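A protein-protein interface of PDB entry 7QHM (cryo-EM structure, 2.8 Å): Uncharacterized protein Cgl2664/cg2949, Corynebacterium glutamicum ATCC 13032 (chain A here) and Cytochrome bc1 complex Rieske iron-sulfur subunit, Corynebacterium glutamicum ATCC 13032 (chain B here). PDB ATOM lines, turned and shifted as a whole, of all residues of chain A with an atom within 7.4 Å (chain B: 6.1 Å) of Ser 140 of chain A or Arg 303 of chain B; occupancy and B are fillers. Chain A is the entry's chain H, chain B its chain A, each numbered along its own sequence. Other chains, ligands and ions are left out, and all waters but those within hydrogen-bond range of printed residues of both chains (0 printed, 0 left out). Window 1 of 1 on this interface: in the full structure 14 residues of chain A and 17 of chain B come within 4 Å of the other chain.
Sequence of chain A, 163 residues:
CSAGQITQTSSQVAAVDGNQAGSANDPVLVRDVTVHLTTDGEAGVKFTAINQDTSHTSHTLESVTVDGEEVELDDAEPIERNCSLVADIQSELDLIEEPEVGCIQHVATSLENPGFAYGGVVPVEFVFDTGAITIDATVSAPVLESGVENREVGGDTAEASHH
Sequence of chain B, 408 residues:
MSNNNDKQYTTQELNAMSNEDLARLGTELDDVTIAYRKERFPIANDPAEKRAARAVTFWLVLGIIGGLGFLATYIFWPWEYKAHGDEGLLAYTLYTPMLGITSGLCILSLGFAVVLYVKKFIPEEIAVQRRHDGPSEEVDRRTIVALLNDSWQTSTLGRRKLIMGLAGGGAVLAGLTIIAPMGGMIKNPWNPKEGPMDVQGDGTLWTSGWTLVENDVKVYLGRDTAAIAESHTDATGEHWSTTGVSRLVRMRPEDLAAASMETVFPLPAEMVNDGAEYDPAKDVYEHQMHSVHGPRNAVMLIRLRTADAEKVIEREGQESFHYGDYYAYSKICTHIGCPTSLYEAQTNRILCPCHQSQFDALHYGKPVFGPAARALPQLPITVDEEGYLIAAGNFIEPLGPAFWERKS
The side-chain carboxylate of Asp 17 of chain A is in hydrogen-bond range of the backbone NH of Ala 258 of chain B, 3.1 Å away.
The side-chain hydroxyl (OG1) of Thr 138 of chain A lies within hydrogen-bond range of the guanidinium group (NH2) of Arg 303 of chain B, at 2.9 Å.
NH2 of Arg 303 of chain B sits at hydrogen-bond distance from O of Val 139 of chain A, 3.0 Å away.
O of Gly 119 of chain A lies within hydrogen-bond range of N of Asp 325 of chain B (3.2 Å).
N of Arg 303 of chain B is in hydrogen-bond range of O of Ser 260 of chain B.
The backbone NH of Leu 304 of chain B lies within hydrogen-bond range of the backbone carbonyl oxygen of Asp 325 of chain B (3.1 Å).
The side-chain carboxylate of Asp 17 of chain A sits at hydrogen-bond distance from the side-chain hydroxyl of Ser 140 of chain A, 2.8 Å away.
The backbone carbonyl oxygen (O) of Thr 138 of chain A lies within hydrogen-bond range of the side-chain hydroxyl (OG1) of Thr 34 of chain A.
The backbone NH (N) of Val 35 of chain A lies within hydrogen-bond range of the backbone carbonyl oxygen (O) of Thr 138 of chain A (3.0 Å).
N of Leu 37 of chain A sits at hydrogen-bond distance from O of Ser 140 of chain A (3.0 Å).
CB of Ala 257 of chain B touches OD1 of Asp 17 of chain A (3.6 Å).
C of Pro 253 of chain B touches CB of Tyr 118 of chain A (3.997 Å).
Tyr 118 of chain A touches Glu 254 of chain B (CD2 to OE1, 3.5 Å).
Tyr 326 of chain B touches Gly 119 of chain A (CE2 to CA, 3.7 Å).
Val 121 of chain A touches Asp 325 of chain B.
Ser 140 of chain A touches Arg 303 of chain B (OG to NH1, 3.8 Å).
Of the printed residues of chain B, Tyr 118 of chain A touches Pro 253 and Glu 254.
Printed residues of chain B within 4 Å of Gly 119 of chain A: Asp 325 and Tyr 326.
Of the printed residues of chain B, Thr 138 of chain A touches Arg 303 (2.9 Å).
Of chain B, only Arg 303 (3.8 Å) comes within 4 Å of Ser 140 of chain A.
Of the printed residues of chain A, Pro 253 of chain B touches Tyr 118.
Of chain A, only Thr 138, Val 139 and Ser 140 come within 4 Å of Arg 303 of chain B.
Hydrophobic or aromatic side chains of chain B within 4 Å of the printed part of chain A: Ala 257, Ala 258 and Tyr 326.
Printed residues of chain A that touch a printed residue of chain B: Asp 17, Tyr 118, Gly 119, Val 121, Thr 138, Val 139 and Ser 140.
Hydrophobic or aromatic side chains of chain A within 4 Å of the printed part of chain B: Tyr 118 and Val 121.
Along chain A the printed residues that touch a printed residue of chain B span positions 17 to 140.
Among the printed residues, 10 pairs touch across the chains.
Among the printed residues, no Asp or Glu carboxylate lies within 4 Å of a Lys or Arg side-chain nitrogen of the other chain.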
ATOM      1  N   ASP A  17     -23.618  19.281  27.077  1.00  0.00           N
ATOM      2  CA  ASP A  17     -23.509  20.389  28.020  1.00  0.00           C
ATOM      3  C   ASP A  17     -24.204  20.080  29.339  1.00  0.00           C
ATOM      4  O   ASP A  17     -23.766  20.553  30.393  1.00  0.00           O
ATOM      5  CB  ASP A  17     -24.098  21.662  27.414  1.00  0.00           C
ATOM      6  CG  ASP A  17     -23.187  22.293  26.383  1.00  0.00           C
ATOM      7  OD1 ASP A  17     -22.243  21.613  25.930  1.00  0.00           O
ATOM      8  OD2 ASP A  17     -23.407  23.470  26.031  1.00  0.00           O
ATOM      9  N   GLY A  18     -25.276  19.294  29.305  1.00  0.00           N
ATOM     10  CA  GLY A  18     -26.060  19.075  30.499  1.00  0.00           C
ATOM     11  C   GLY A  18     -25.401  18.105  31.459  1.00  0.00           C
ATOM     12  O   GLY A  18     -24.733  17.154  31.063  1.00  0.00           O
ATOM     13  N   THR A  34     -29.379  21.190  31.954  1.00  0.00           N
ATOM     14  CA  THR A  34     -28.775  22.487  31.689  1.00  0.00           C
ATOM     15  C   THR A  34     -29.864  23.547  31.681  1.00  0.00           C
ATOM     16  O   THR A  34     -31.047  23.245  31.521  1.00  0.00           O
ATOM     17  CB  THR A  34     -27.993  22.512  30.366  1.00  0.00           C
ATOM     18  OG1 THR A  34     -27.594  23.856  30.072  1.00  0.00           O
ATOM     19  CG2 THR A  34     -28.814  21.977  29.215  1.00  0.00           C
ATOM     20  N   VAL A  35     -29.450  24.794  31.882  1.00  0.00           N
ATOM     21  CA  VAL A  35     -30.346  25.942  31.854  1.00  0.00           C
ATOM     22  C   VAL A  35     -30.159  26.609  30.499  1.00  0.00           C
ATOM     23  O   VAL A  35     -29.254  27.422  30.312  1.00  0.00           O
ATOM     24  CB  VAL A  35     -30.076  26.912  33.006  1.00  0.00           C
ATOM     25  CG1 VAL A  35     -30.809  28.240  32.775  1.00  0.00           C
ATOM     26  CG2 VAL A  35     -30.509  26.287  34.329  1.00  0.00           C
ATOM     27  N   HIS A  36     -31.019  26.258  29.553  1.00  0.00           N
ATOM     28  CA  HIS A  36     -30.976  26.881  28.242  1.00  0.00           C
ATOM     29  C   HIS A  36     -31.464  28.316  28.325  1.00  0.00           C
ATOM     30  O   HIS A  36     -32.469  28.613  28.974  1.00  0.00           O
ATOM     31  CB  HIS A  36     -31.819  26.090  27.245  1.00  0.00           C
ATOM     32  CG  HIS A  36     -31.080  24.972  26.578  1.00  0.00           C
ATOM     33  ND1 HIS A  36     -31.571  24.314  25.474  1.00  0.00           N
ATOM     34  CD2 HIS A  36     -29.884  24.400  26.853  1.00  0.00           C
ATOM     35  CE1 HIS A  36     -30.710  23.389  25.094  1.00  0.00           C
ATOM     36  NE2 HIS A  36     -29.678  23.418  25.918  1.00  0.00           N
ATOM     37  N   LEU A  37     -30.722  29.210  27.673  1.00  0.00           N
ATOM     38  CA  LEU A  37     -30.992  30.642  27.655  1.00  0.00           C
ATOM     39  C   LEU A  37     -30.866  31.085  26.205  1.00  0.00           C
ATOM     40  O   LEU A  37     -29.766  31.375  25.732  1.00  0.00           O
ATOM     41  CB  LEU A  37     -30.026  31.393  28.572  1.00  0.00           C
ATOM     42  CG  LEU A  37     -30.017  32.927  28.512  1.00  0.00           C
ATOM     43  CD1 LEU A  37     -31.372  33.504  28.895  1.00  0.00           C
ATOM     44  CD2 LEU A  37     -28.920  33.497  29.405  1.00  0.00           C
ATOM     45  N   THR A  38     -31.989  31.129  25.496  1.00  0.00           N
ATOM     46  CA  THR A  38     -31.981  31.668  24.145  1.00  0.00           C
ATOM     47  C   THR A  38     -31.587  33.139  24.177  1.00  0.00           C
ATOM     48  O   THR A  38     -31.854  33.856  25.145  1.00  0.00           O
ATOM     49  CB  THR A  38     -33.355  31.508  23.498  1.00  0.00           C
ATOM     50  OG1 THR A  38     -33.889  30.217  23.818  1.00  0.00           O
ATOM     51  CG2 THR A  38     -33.260  31.649  21.986  1.00  0.00           C
ATOM     52  N   GLY A  44     -35.176  28.458  30.033  1.00  0.00           N
ATOM     53  CA  GLY A  44     -35.814  27.331  30.683  1.00  0.00           C
ATOM     54  C   GLY A  44     -34.834  26.206  30.897  1.00  0.00           C
ATOM     55  O   GLY A  44     -33.707  26.227  30.412  1.00  0.00           O
ATOM     56  N   ILE A  89     -37.189  23.770  26.474  1.00  0.00           N
ATOM     57  CA  ILE A  89     -37.822  25.014  26.018  1.00  0.00           C
ATOM     58  C   ILE A  89     -38.514  24.781  24.676  1.00  0.00           C
ATOM     59  O   ILE A  89     -38.160  23.882  23.905  1.00  0.00           O
ATOM     60  CB  ILE A  89     -36.812  26.174  25.927  1.00  0.00           C
ATOM     61  CG1 ILE A  89     -35.574  25.790  25.100  1.00  0.00           C
ATOM     62  CG2 ILE A  89     -36.403  26.615  27.311  1.00  0.00           C
ATOM     63  CD1 ILE A  89     -34.734  26.971  24.654  1.00  0.00           C
ATOM     64  N   ALA A 117     -26.187  34.453  33.105  1.00  0.00           N
ATOM     65  CA  ALA A 117     -25.259  34.724  32.021  1.00  0.00           C
ATOM     66  C   ALA A 117     -24.483  33.457  31.714  1.00  0.00           C
ATOM     67  O   ALA A 117     -24.291  32.601  32.581  1.00  0.00           O
ATOM     68  CB  ALA A 117     -24.288  35.860  32.357  1.00  0.00           C
ATOM     69  N   TYR A 118     -24.027  33.362  30.471  1.00  0.00           N
ATOM     70  CA  TYR A 118     -23.436  32.138  29.970  1.00  0.00           C
ATOM     71  C   TYR A 118     -22.106  31.860  30.657  1.00  0.00           C
ATOM     72  O   TYR A 118     -21.469  32.749  31.228  1.00  0.00           O
ATOM     73  CB  TYR A 118     -23.235  32.227  28.461  1.00  0.00           C
ATOM     74  CG  TYR A 118     -24.512  32.474  27.704  1.00  0.00           C
ATOM     75  CD1 TYR A 118     -25.449  31.471  27.551  1.00  0.00           C
ATOM     76  CD2 TYR A 118     -24.784  33.710  27.151  1.00  0.00           C
ATOM     77  CE1 TYR A 118     -26.611  31.689  26.869  1.00  0.00           C
ATOM     78  CE2 TYR A 118     -25.946  33.935  26.464  1.00  0.00           C
ATOM     79  CZ  TYR A 118     -26.857  32.918  26.327  1.00  0.00           C
ATOM     80  OH  TYR A 118     -28.026  33.135  25.641  1.00  0.00           O
ATOM     81  N   GLY A 119     -21.697  30.605  30.592  1.00  0.00           N
ATOM     82  CA  GLY A 119     -20.437  30.153  31.154  1.00  0.00           C
ATOM     83  C   GLY A 119     -20.552  29.606  32.550  1.00  0.00           C
ATOM     84  O   GLY A 119     -20.022  28.537  32.849  1.00  0.00           O
ATOM     85  N   GLY A 120     -21.251  30.321  33.419  1.00  0.00           N
ATOM     86  CA  GLY A 120     -21.349  29.924  34.803  1.00  0.00           C
ATOM     87  C   GLY A 120     -22.273  28.737  34.986  1.00  0.00           C
ATOM     88  O   GLY A 120     -22.698  28.072  34.043  1.00  0.00           O
ATOM     89  N   VAL A 121     -22.586  28.471  36.254  1.00  0.00           N
ATOM     90  CA  VAL A 121     -23.485  27.393  36.635  1.00  0.00           C
ATOM     91  C   VAL A 121     -24.409  27.897  37.734  1.00  0.00           C
ATOM     92  O   VAL A 121     -24.126  28.887  38.412  1.00  0.00           O
ATOM     93  CB  VAL A 121     -22.733  26.124  37.104  1.00  0.00           C
ATOM     94  CG1 VAL A 121     -21.816  25.608  36.011  1.00  0.00           C
ATOM     95  CG2 VAL A 121     -21.936  26.394  38.373  1.00  0.00           C
ATOM     96  N   ALA A 137     -26.202  22.963  37.286  1.00  0.00           N
ATOM     97  CA  ALA A 137     -26.479  22.988  35.857  1.00  0.00           C
ATOM     98  C   ALA A 137     -25.870  24.232  35.233  1.00  0.00           C
ATOM     99  O   ALA A 137     -25.994  25.328  35.782  1.00  0.00           O
ATOM    100  CB  ALA A 137     -27.985  22.974  35.600  1.00  0.00           C
ATOM    101  N   THR A 138     -25.227  24.071  34.082  1.00  0.00           N
ATOM    102  CA  THR A 138     -24.595  25.209  33.431  1.00  0.00           C
ATOM    103  C   THR A 138     -25.604  25.974  32.591  1.00  0.00           C
ATOM    104  O   THR A 138     -26.543  25.403  32.032  1.00  0.00           O
ATOM    105  CB  THR A 138     -23.407  24.773  32.562  1.00  0.00           C
ATOM    106  OG1 THR A 138     -22.714  25.930  32.083  1.00  0.00           O
ATOM    107  CG2 THR A 138     -23.840  23.930  31.368  1.00  0.00           C
ATOM    108  N   VAL A 139     -25.409  27.283  32.525  1.00  0.00           N
ATOM    109  CA  VAL A 139     -26.160  28.121  31.604  1.00  0.00           C
ATOM    110  C   VAL A 139     -25.500  28.007  30.240  1.00  0.00           C
ATOM    111  O   VAL A 139     -24.276  28.132  30.121  1.00  0.00           O
ATOM    112  CB  VAL A 139     -26.203  29.577  32.094  1.00  0.00           C
ATOM    113  CG1 VAL A 139     -27.075  30.435  31.187  1.00  0.00           C
ATOM    114  CG2 VAL A 139     -26.711  29.641  33.528  1.00  0.00           C
ATOM    115  N   SER A 140     -26.303  27.751  29.211  1.00  0.00           N
ATOM    116  CA  SER A 140     -25.770  27.549  27.874  1.00  0.00           C
ATOM    117  C   SER A 140     -26.800  27.992  26.849  1.00  0.00           C
ATOM    118  O   SER A 140     -27.993  28.094  27.140  1.00  0.00           O
ATOM    119  CB  SER A 140     -25.388  26.084  27.644  1.00  0.00           C
ATOM    120  OG  SER A 140     -24.622  25.937  26.464  1.00  0.00           O
ATOM    121  N   ALA A 141     -26.318  28.260  25.644  1.00  0.00           N
ATOM    122  CA  ALA A 141     -27.203  28.569  24.535  1.00  0.00           C
ATOM    123  C   ALA A 141     -27.683  27.274  23.883  1.00  0.00           C
ATOM    124  O   ALA A 141     -26.911  26.312  23.791  1.00  0.00           O
ATOM    125  CB  ALA A 141     -26.485  29.422  23.499  1.00  0.00           C
ATOM    126  N   PRO A 142     -28.936  27.165  23.432  1.00  0.00           N
ATOM    127  CA  PRO A 142     -29.332  25.977  22.673  1.00  0.00           C
ATOM    128  C   PRO A 142     -28.479  25.790  21.426  1.00  0.00           C
ATOM    129  O   PRO A 142     -27.817  26.711  20.943  1.00  0.00           O
ATOM    130  CB  PRO A 142     -30.793  26.260  22.312  1.00  0.00           C
ATOM    131  CG  PRO A 142     -31.264  27.157  23.377  1.00  0.00           C
ATOM    132  CD  PRO A 142     -30.097  28.022  23.724  1.00  0.00           C
ATOM    133  N   VAL A 143     -28.497  24.566  20.911  1.00  0.00           N
ATOM    134  CA  VAL A 143     -27.666  24.200  19.770  1.00  0.00           C
ATOM    135  C   VAL A 143     -28.278  24.773  18.500  1.00  0.00           C
ATOM    136  O   VAL A 143     -29.502  24.794  18.333  1.00  0.00           O
ATOM    137  CB  VAL A 143     -27.511  22.669  19.684  1.00  0.00           C
ATOM    138  CG1 VAL A 143     -26.637  22.274  18.498  1.00  0.00           C
ATOM    139  CG2 VAL A 143     -26.916  22.117  20.979  1.00  0.00           C
ATOM    140  N   PRO B 253     -19.071  34.412  25.640  1.00  0.00           N
ATOM    141  CA  PRO B 253     -19.077  33.192  26.462  1.00  0.00           C
ATOM    142  C   PRO B 253     -20.073  32.139  26.017  1.00  0.00           C
ATOM    143  O   PRO B 253     -19.944  30.986  26.444  1.00  0.00           O
ATOM    144  CB  PRO B 253     -19.409  33.710  27.867  1.00  0.00           C
ATOM    145  CG  PRO B 253     -20.049  35.008  27.655  1.00  0.00           C
ATOM    146  CD  PRO B 253     -19.438  35.595  26.434  1.00  0.00           C
ATOM    147  N   GLU B 254     -21.053  32.471  25.184  1.00  0.00           N
ATOM    148  CA  GLU B 254     -21.988  31.457  24.712  1.00  0.00           C
ATOM    149  C   GLU B 254     -21.388  30.541  23.662  1.00  0.00           C
ATOM    150  O   GLU B 254     -21.991  29.511  23.347  1.00  0.00           O
ATOM    151  CB  GLU B 254     -23.250  32.105  24.128  1.00  0.00           C
ATOM    152  CG  GLU B 254     -23.018  33.116  23.006  1.00  0.00           C
ATOM    153  CD  GLU B 254     -22.939  34.542  23.499  1.00  0.00           C
ATOM    154  OE1 GLU B 254     -22.526  34.758  24.656  1.00  0.00           O
ATOM    155  OE2 GLU B 254     -23.293  35.454  22.729  1.00  0.00           O
ATOM    156  N   ASP B 255     -20.220  30.879  23.125  1.00  0.00           N
ATOM    157  CA  ASP B 255     -19.793  30.295  21.862  1.00  0.00           C
ATOM    158  C   ASP B 255     -19.346  28.852  22.025  1.00  0.00           C
ATOM    159  O   ASP B 255     -19.686  27.999  21.201  1.00  0.00           O
ATOM    160  CB  ASP B 255     -18.679  31.147  21.263  1.00  0.00           C
ATOM    161  CG  ASP B 255     -19.194  32.449  20.678  1.00  0.00           C
ATOM    162  OD1 ASP B 255     -20.397  32.733  20.817  1.00  0.00           O
ATOM    163  OD2 ASP B 255     -18.402  33.188  20.063  1.00  0.00           O
ATOM    164  N   LEU B 256     -18.594  28.555  23.072  1.00  0.00           N
ATOM    165  CA  LEU B 256     -17.978  27.249  23.219  1.00  0.00           C
ATOM    166  C   LEU B 256     -18.887  26.318  24.005  1.00  0.00           C
ATOM    167  O   LEU B 256     -19.299  26.642  25.121  1.00  0.00           O
ATOM    168  CB  LEU B 256     -16.630  27.377  23.922  1.00  0.00           C
ATOM    169  CG  LEU B 256     -15.569  28.301  23.330  1.00  0.00           C
ATOM    170  CD1 LEU B 256     -14.240  27.991  23.959  1.00  0.00           C
ATOM    171  CD2 LEU B 256     -15.469  28.183  21.834  1.00  0.00           C
ATOM    172  N   ALA B 257     -19.189  25.162  23.427  1.00  0.00           N
ATOM    173  CA  ALA B 257     -19.835  24.108  24.184  1.00  0.00           C
ATOM    174  C   ALA B 257     -18.907  23.631  25.291  1.00  0.00           C
ATOM    175  O   ALA B 257     -17.725  23.960  25.331  1.00  0.00           O
ATOM    176  CB  ALA B 257     -20.203  22.936  23.279  1.00  0.00           C
ATOM    177  N   ALA B 258     -19.458  22.858  26.214  1.00  0.00           N
ATOM    178  CA  ALA B 258     -18.611  22.241  27.219  1.00  0.00           C
ATOM    179  C   ALA B 258     -17.653  21.264  26.549  1.00  0.00           C
ATOM    180  O   ALA B 258     -17.981  20.626  25.546  1.00  0.00           O
ATOM    181  CB  ALA B 258     -19.459  21.530  28.270  1.00  0.00           C
ATOM    182  N   ALA B 259     -16.450  21.165  27.109  1.00  0.00           N
ATOM    183  CA  ALA B 259     -15.367  20.368  26.533  1.00  0.00           C
ATOM    184  C   ALA B 259     -15.021  20.836  25.123  1.00  0.00           C
ATOM    185  O   ALA B 259     -14.758  20.028  24.231  1.00  0.00           O
ATOM    186  CB  ALA B 259     -15.700  18.877  26.543  1.00  0.00           C
ATOM    187  N   SER B 260     -15.031  22.151  24.921  1.00  0.00           N
ATOM    188  CA  SER B 260     -14.460  22.792  23.750  1.00  0.00           C
ATOM    189  C   SER B 260     -13.202  23.547  24.147  1.00  0.00           C
ATOM    190  O   SER B 260     -13.008  23.910  25.311  1.00  0.00           O
ATOM    191  CB  SER B 260     -15.441  23.763  23.095  1.00  0.00           C
ATOM    192  OG  SER B 260     -16.428  23.086  22.342  1.00  0.00           O
ATOM    193  N   MET B 261     -12.351  23.777  23.150  1.00  0.00           N
ATOM    194  CA  MET B 261     -11.119  24.533  23.299  1.00  0.00           C
ATOM    195  C   MET B 261     -10.988  25.476  22.116  1.00  0.00           C
ATOM    196  O   MET B 261     -11.232  25.086  20.974  1.00  0.00           O
ATOM    197  CB  MET B 261      -9.909  23.596  23.384  1.00  0.00           C
ATOM    198  CG  MET B 261      -8.559  24.273  23.257  1.00  0.00           C
ATOM    199  SD  MET B 261      -7.932  24.275  21.564  1.00  0.00           S
ATOM    200  CE  MET B 261      -6.494  25.331  21.694  1.00  0.00           C
ATOM    201  N   LEU B 301      -8.174  28.553  25.609  1.00  0.00           N
ATOM    202  CA  LEU B 301      -9.389  28.848  26.363  1.00  0.00           C
ATOM    203  C   LEU B 301     -10.291  27.626  26.305  1.00  0.00           C
ATOM    204  O   LEU B 301     -10.849  27.317  25.248  1.00  0.00           O
ATOM    205  CB  LEU B 301     -10.096  30.070  25.787  1.00  0.00           C
ATOM    206  CG  LEU B 301     -11.432  30.504  26.387  1.00  0.00           C
ATOM    207  CD1 LEU B 301     -11.214  31.176  27.714  1.00  0.00           C
ATOM    208  CD2 LEU B 301     -12.149  31.426  25.437  1.00  0.00           C
ATOM    209  N   ILE B 302     -10.448  26.955  27.440  1.00  0.00           N
ATOM    210  CA  ILE B 302     -11.203  25.713  27.533  1.00  0.00           C
ATOM    211  C   ILE B 302     -12.491  25.991  28.284  1.00  0.00           C
ATOM    212  O   ILE B 302     -12.540  26.846  29.174  1.00  0.00           O
ATOM    213  CB  ILE B 302     -10.372  24.614  28.225  1.00  0.00           C
ATOM    214  CG1 ILE B 302      -9.215  24.195  27.322  1.00  0.00           C
ATOM    215  CG2 ILE B 302     -11.223  23.393  28.543  1.00  0.00           C
ATOM    216  CD1 ILE B 302      -8.075  23.534  28.038  1.00  0.00           C
ATOM    217  N   ARG B 303     -13.550  25.285  27.900  1.00  0.00           N
ATOM    218  CA  ARG B 303     -14.768  25.209  28.698  1.00  0.00           C
ATOM    219  C   ARG B 303     -14.888  23.798  29.253  1.00  0.00           C
ATOM    220  O   ARG B 303     -15.003  22.837  28.487  1.00  0.00           O
ATOM    221  CB  ARG B 303     -16.007  25.574  27.883  1.00  0.00           C
ATOM    222  CG  ARG B 303     -17.247  25.668  28.737  1.00  0.00           C
ATOM    223  CD  ARG B 303     -18.460  26.132  27.981  1.00  0.00           C
ATOM    224  NE  ARG B 303     -19.596  26.245  28.882  1.00  0.00           N
ATOM    225  CZ  ARG B 303     -20.804  26.657  28.537  1.00  0.00           C
ATOM    226  NH1 ARG B 303     -21.089  27.016  27.294  1.00  0.00           N
ATOM    227  NH2 ARG B 303     -21.754  26.721  29.466  1.00  0.00           N
ATOM    228  N   LEU B 304     -14.856  23.674  30.575  1.00  0.00           N
ATOM    229  CA  LEU B 304     -15.079  22.390  31.215  1.00  0.00           C
ATOM    230  C   LEU B 304     -16.569  22.084  31.298  1.00  0.00           C
ATOM    231  O   LEU B 304     -17.417  22.976  31.243  1.00  0.00           O
ATOM    232  CB  LEU B 304     -14.498  22.370  32.626  1.00  0.00           C
ATOM    233  CG  LEU B 304     -12.989  22.420  32.820  1.00  0.00           C
ATOM    234  CD1 LEU B 304     -12.682  22.549  34.297  1.00  0.00           C
ATOM    235  CD2 LEU B 304     -12.322  21.197  32.248  1.00  0.00           C
ATOM    236  N   ARG B 305     -16.879  20.797  31.433  1.00  0.00           N
ATOM    237  CA  ARG B 305     -18.221  20.390  31.815  1.00  0.00           C
ATOM    238  C   ARG B 305     -18.438  20.670  33.297  1.00  0.00           C
ATOM    239  O   ARG B 305     -17.493  20.779  34.072  1.00  0.00           O
ATOM    240  CB  ARG B 305     -18.441  18.906  31.553  1.00  0.00           C
ATOM    241  CG  ARG B 305     -18.193  18.455  30.132  1.00  0.00           C
ATOM    242  CD  ARG B 305     -18.356  16.954  30.029  1.00  0.00           C
ATOM    243  NE  ARG B 305     -17.845  16.431  28.771  1.00  0.00           N
ATOM    244  CZ  ARG B 305     -16.574  16.144  28.528  1.00  0.00           C
ATOM    245  NH1 ARG B 305     -15.626  16.341  29.434  1.00  0.00           N
ATOM    246  NH2 ARG B 305     -16.238  15.655  27.339  1.00  0.00           N
ATOM    247  N   ASP B 325     -17.207  28.144  34.251  1.00  0.00           N
ATOM    248  CA  ASP B 325     -16.542  26.945  33.762  1.00  0.00           C
ATOM    249  C   ASP B 325     -15.457  27.238  32.736  1.00  0.00           C
ATOM    250  O   ASP B 325     -14.812  26.298  32.263  1.00  0.00           O
ATOM    251  CB  ASP B 325     -17.572  25.985  33.161  1.00  0.00           C
ATOM    252  CG  ASP B 325     -18.368  25.237  34.219  1.00  0.00           C
ATOM    253  OD1 ASP B 325     -18.174  25.510  35.421  1.00  0.00           O
ATOM    254  OD2 ASP B 325     -19.189  24.370  33.850  1.00  0.00           O
ATOM    255  N   TYR B 326     -15.223  28.502  32.388  1.00  0.00           N
ATOM    256  CA  TYR B 326     -14.203  28.864  31.410  1.00  0.00           C
ATOM    257  C   TYR B 326     -12.855  29.024  32.100  1.00  0.00           C
ATOM    258  O   TYR B 326     -12.725  29.802  33.050  1.00  0.00           O
ATOM    259  CB  TYR B 326     -14.578  30.155  30.691  1.00  0.00           C
ATOM    260  CG  TYR B 326     -15.526  29.954  29.545  1.00  0.00           C
ATOM    261  CD1 TYR B 326     -15.050  29.696  28.272  1.00  0.00           C
ATOM    262  CD2 TYR B 326     -16.894  30.023  29.731  1.00  0.00           C
ATOM    263  CE1 TYR B 326     -15.907  29.512  27.220  1.00  0.00           C
ATOM    264  CE2 TYR B 326     -17.759  29.844  28.686  1.00  0.00           C
ATOM    265  CZ  TYR B 326     -17.264  29.595  27.435  1.00  0.00           C
ATOM    266  OH  TYR B 326     -18.132  29.411  26.391  1.00  0.00           O
ATOM    267  N   TYR B 327     -11.860  28.289  31.620  1.00  0.00           N
ATOM    268  CA  TYR B 327     -10.486  28.399  32.078  1.00  0.00           C
ATOM    269  C   TYR B 327      -9.603  28.816  30.911  1.00  0.00           C
ATOM    270  O   TYR B 327      -9.962  28.643  29.746  1.00  0.00           O
ATOM    271  CB  TYR B 327     -10.003  27.074  32.674  1.00  0.00           C
ATOM    272  CG  TYR B 327     -10.496  26.821  34.076  1.00  0.00           C
ATOM    273  CD1 TYR B 327     -11.802  26.435  34.315  1.00  0.00           C
ATOM    274  CD2 TYR B 327      -9.652  26.970  35.161  1.00  0.00           C
ATOM    275  CE1 TYR B 327     -12.251  26.206  35.589  1.00  0.00           C
ATOM    276  CE2 TYR B 327     -10.091  26.743  36.433  1.00  0.00           C
ATOM    277  CZ  TYR B 327     -11.394  26.360  36.644  1.00  0.00           C
ATOM    278  OH  TYR B 327     -11.839  26.134  37.924  1.00  0.00           O
ATOM    279  N   TYR B 343      -5.933  18.953  23.397  1.00  0.00           N
ATOM    280  CA  TYR B 343      -6.820  18.886  24.555  1.00  0.00           C
ATOM    281  C   TYR B 343      -7.642  17.611  24.460  1.00  0.00           C
ATOM    282  O   TYR B 343      -8.690  17.571  23.817  1.00  0.00           O
ATOM    283  CB  TYR B 343      -7.715  20.114  24.615  1.00  0.00           C
ATOM    284  CG  TYR B 343      -8.806  20.038  25.652  1.00  0.00           C
ATOM    285  CD1 TYR B 343      -8.508  19.832  26.991  1.00  0.00           C
ATOM    286  CD2 TYR B 343     -10.131  20.200  25.296  1.00  0.00           C
ATOM    287  CE1 TYR B 343      -9.501  19.771  27.938  1.00  0.00           C
ATOM    288  CE2 TYR B 343     -11.127  20.145  26.234  1.00  0.00           C
ATOM    289  CZ  TYR B 343     -10.809  19.930  27.557  1.00  0.00           C
ATOM    290  OH  TYR B 343     -11.807  19.871  28.504  1.00  0.00           O
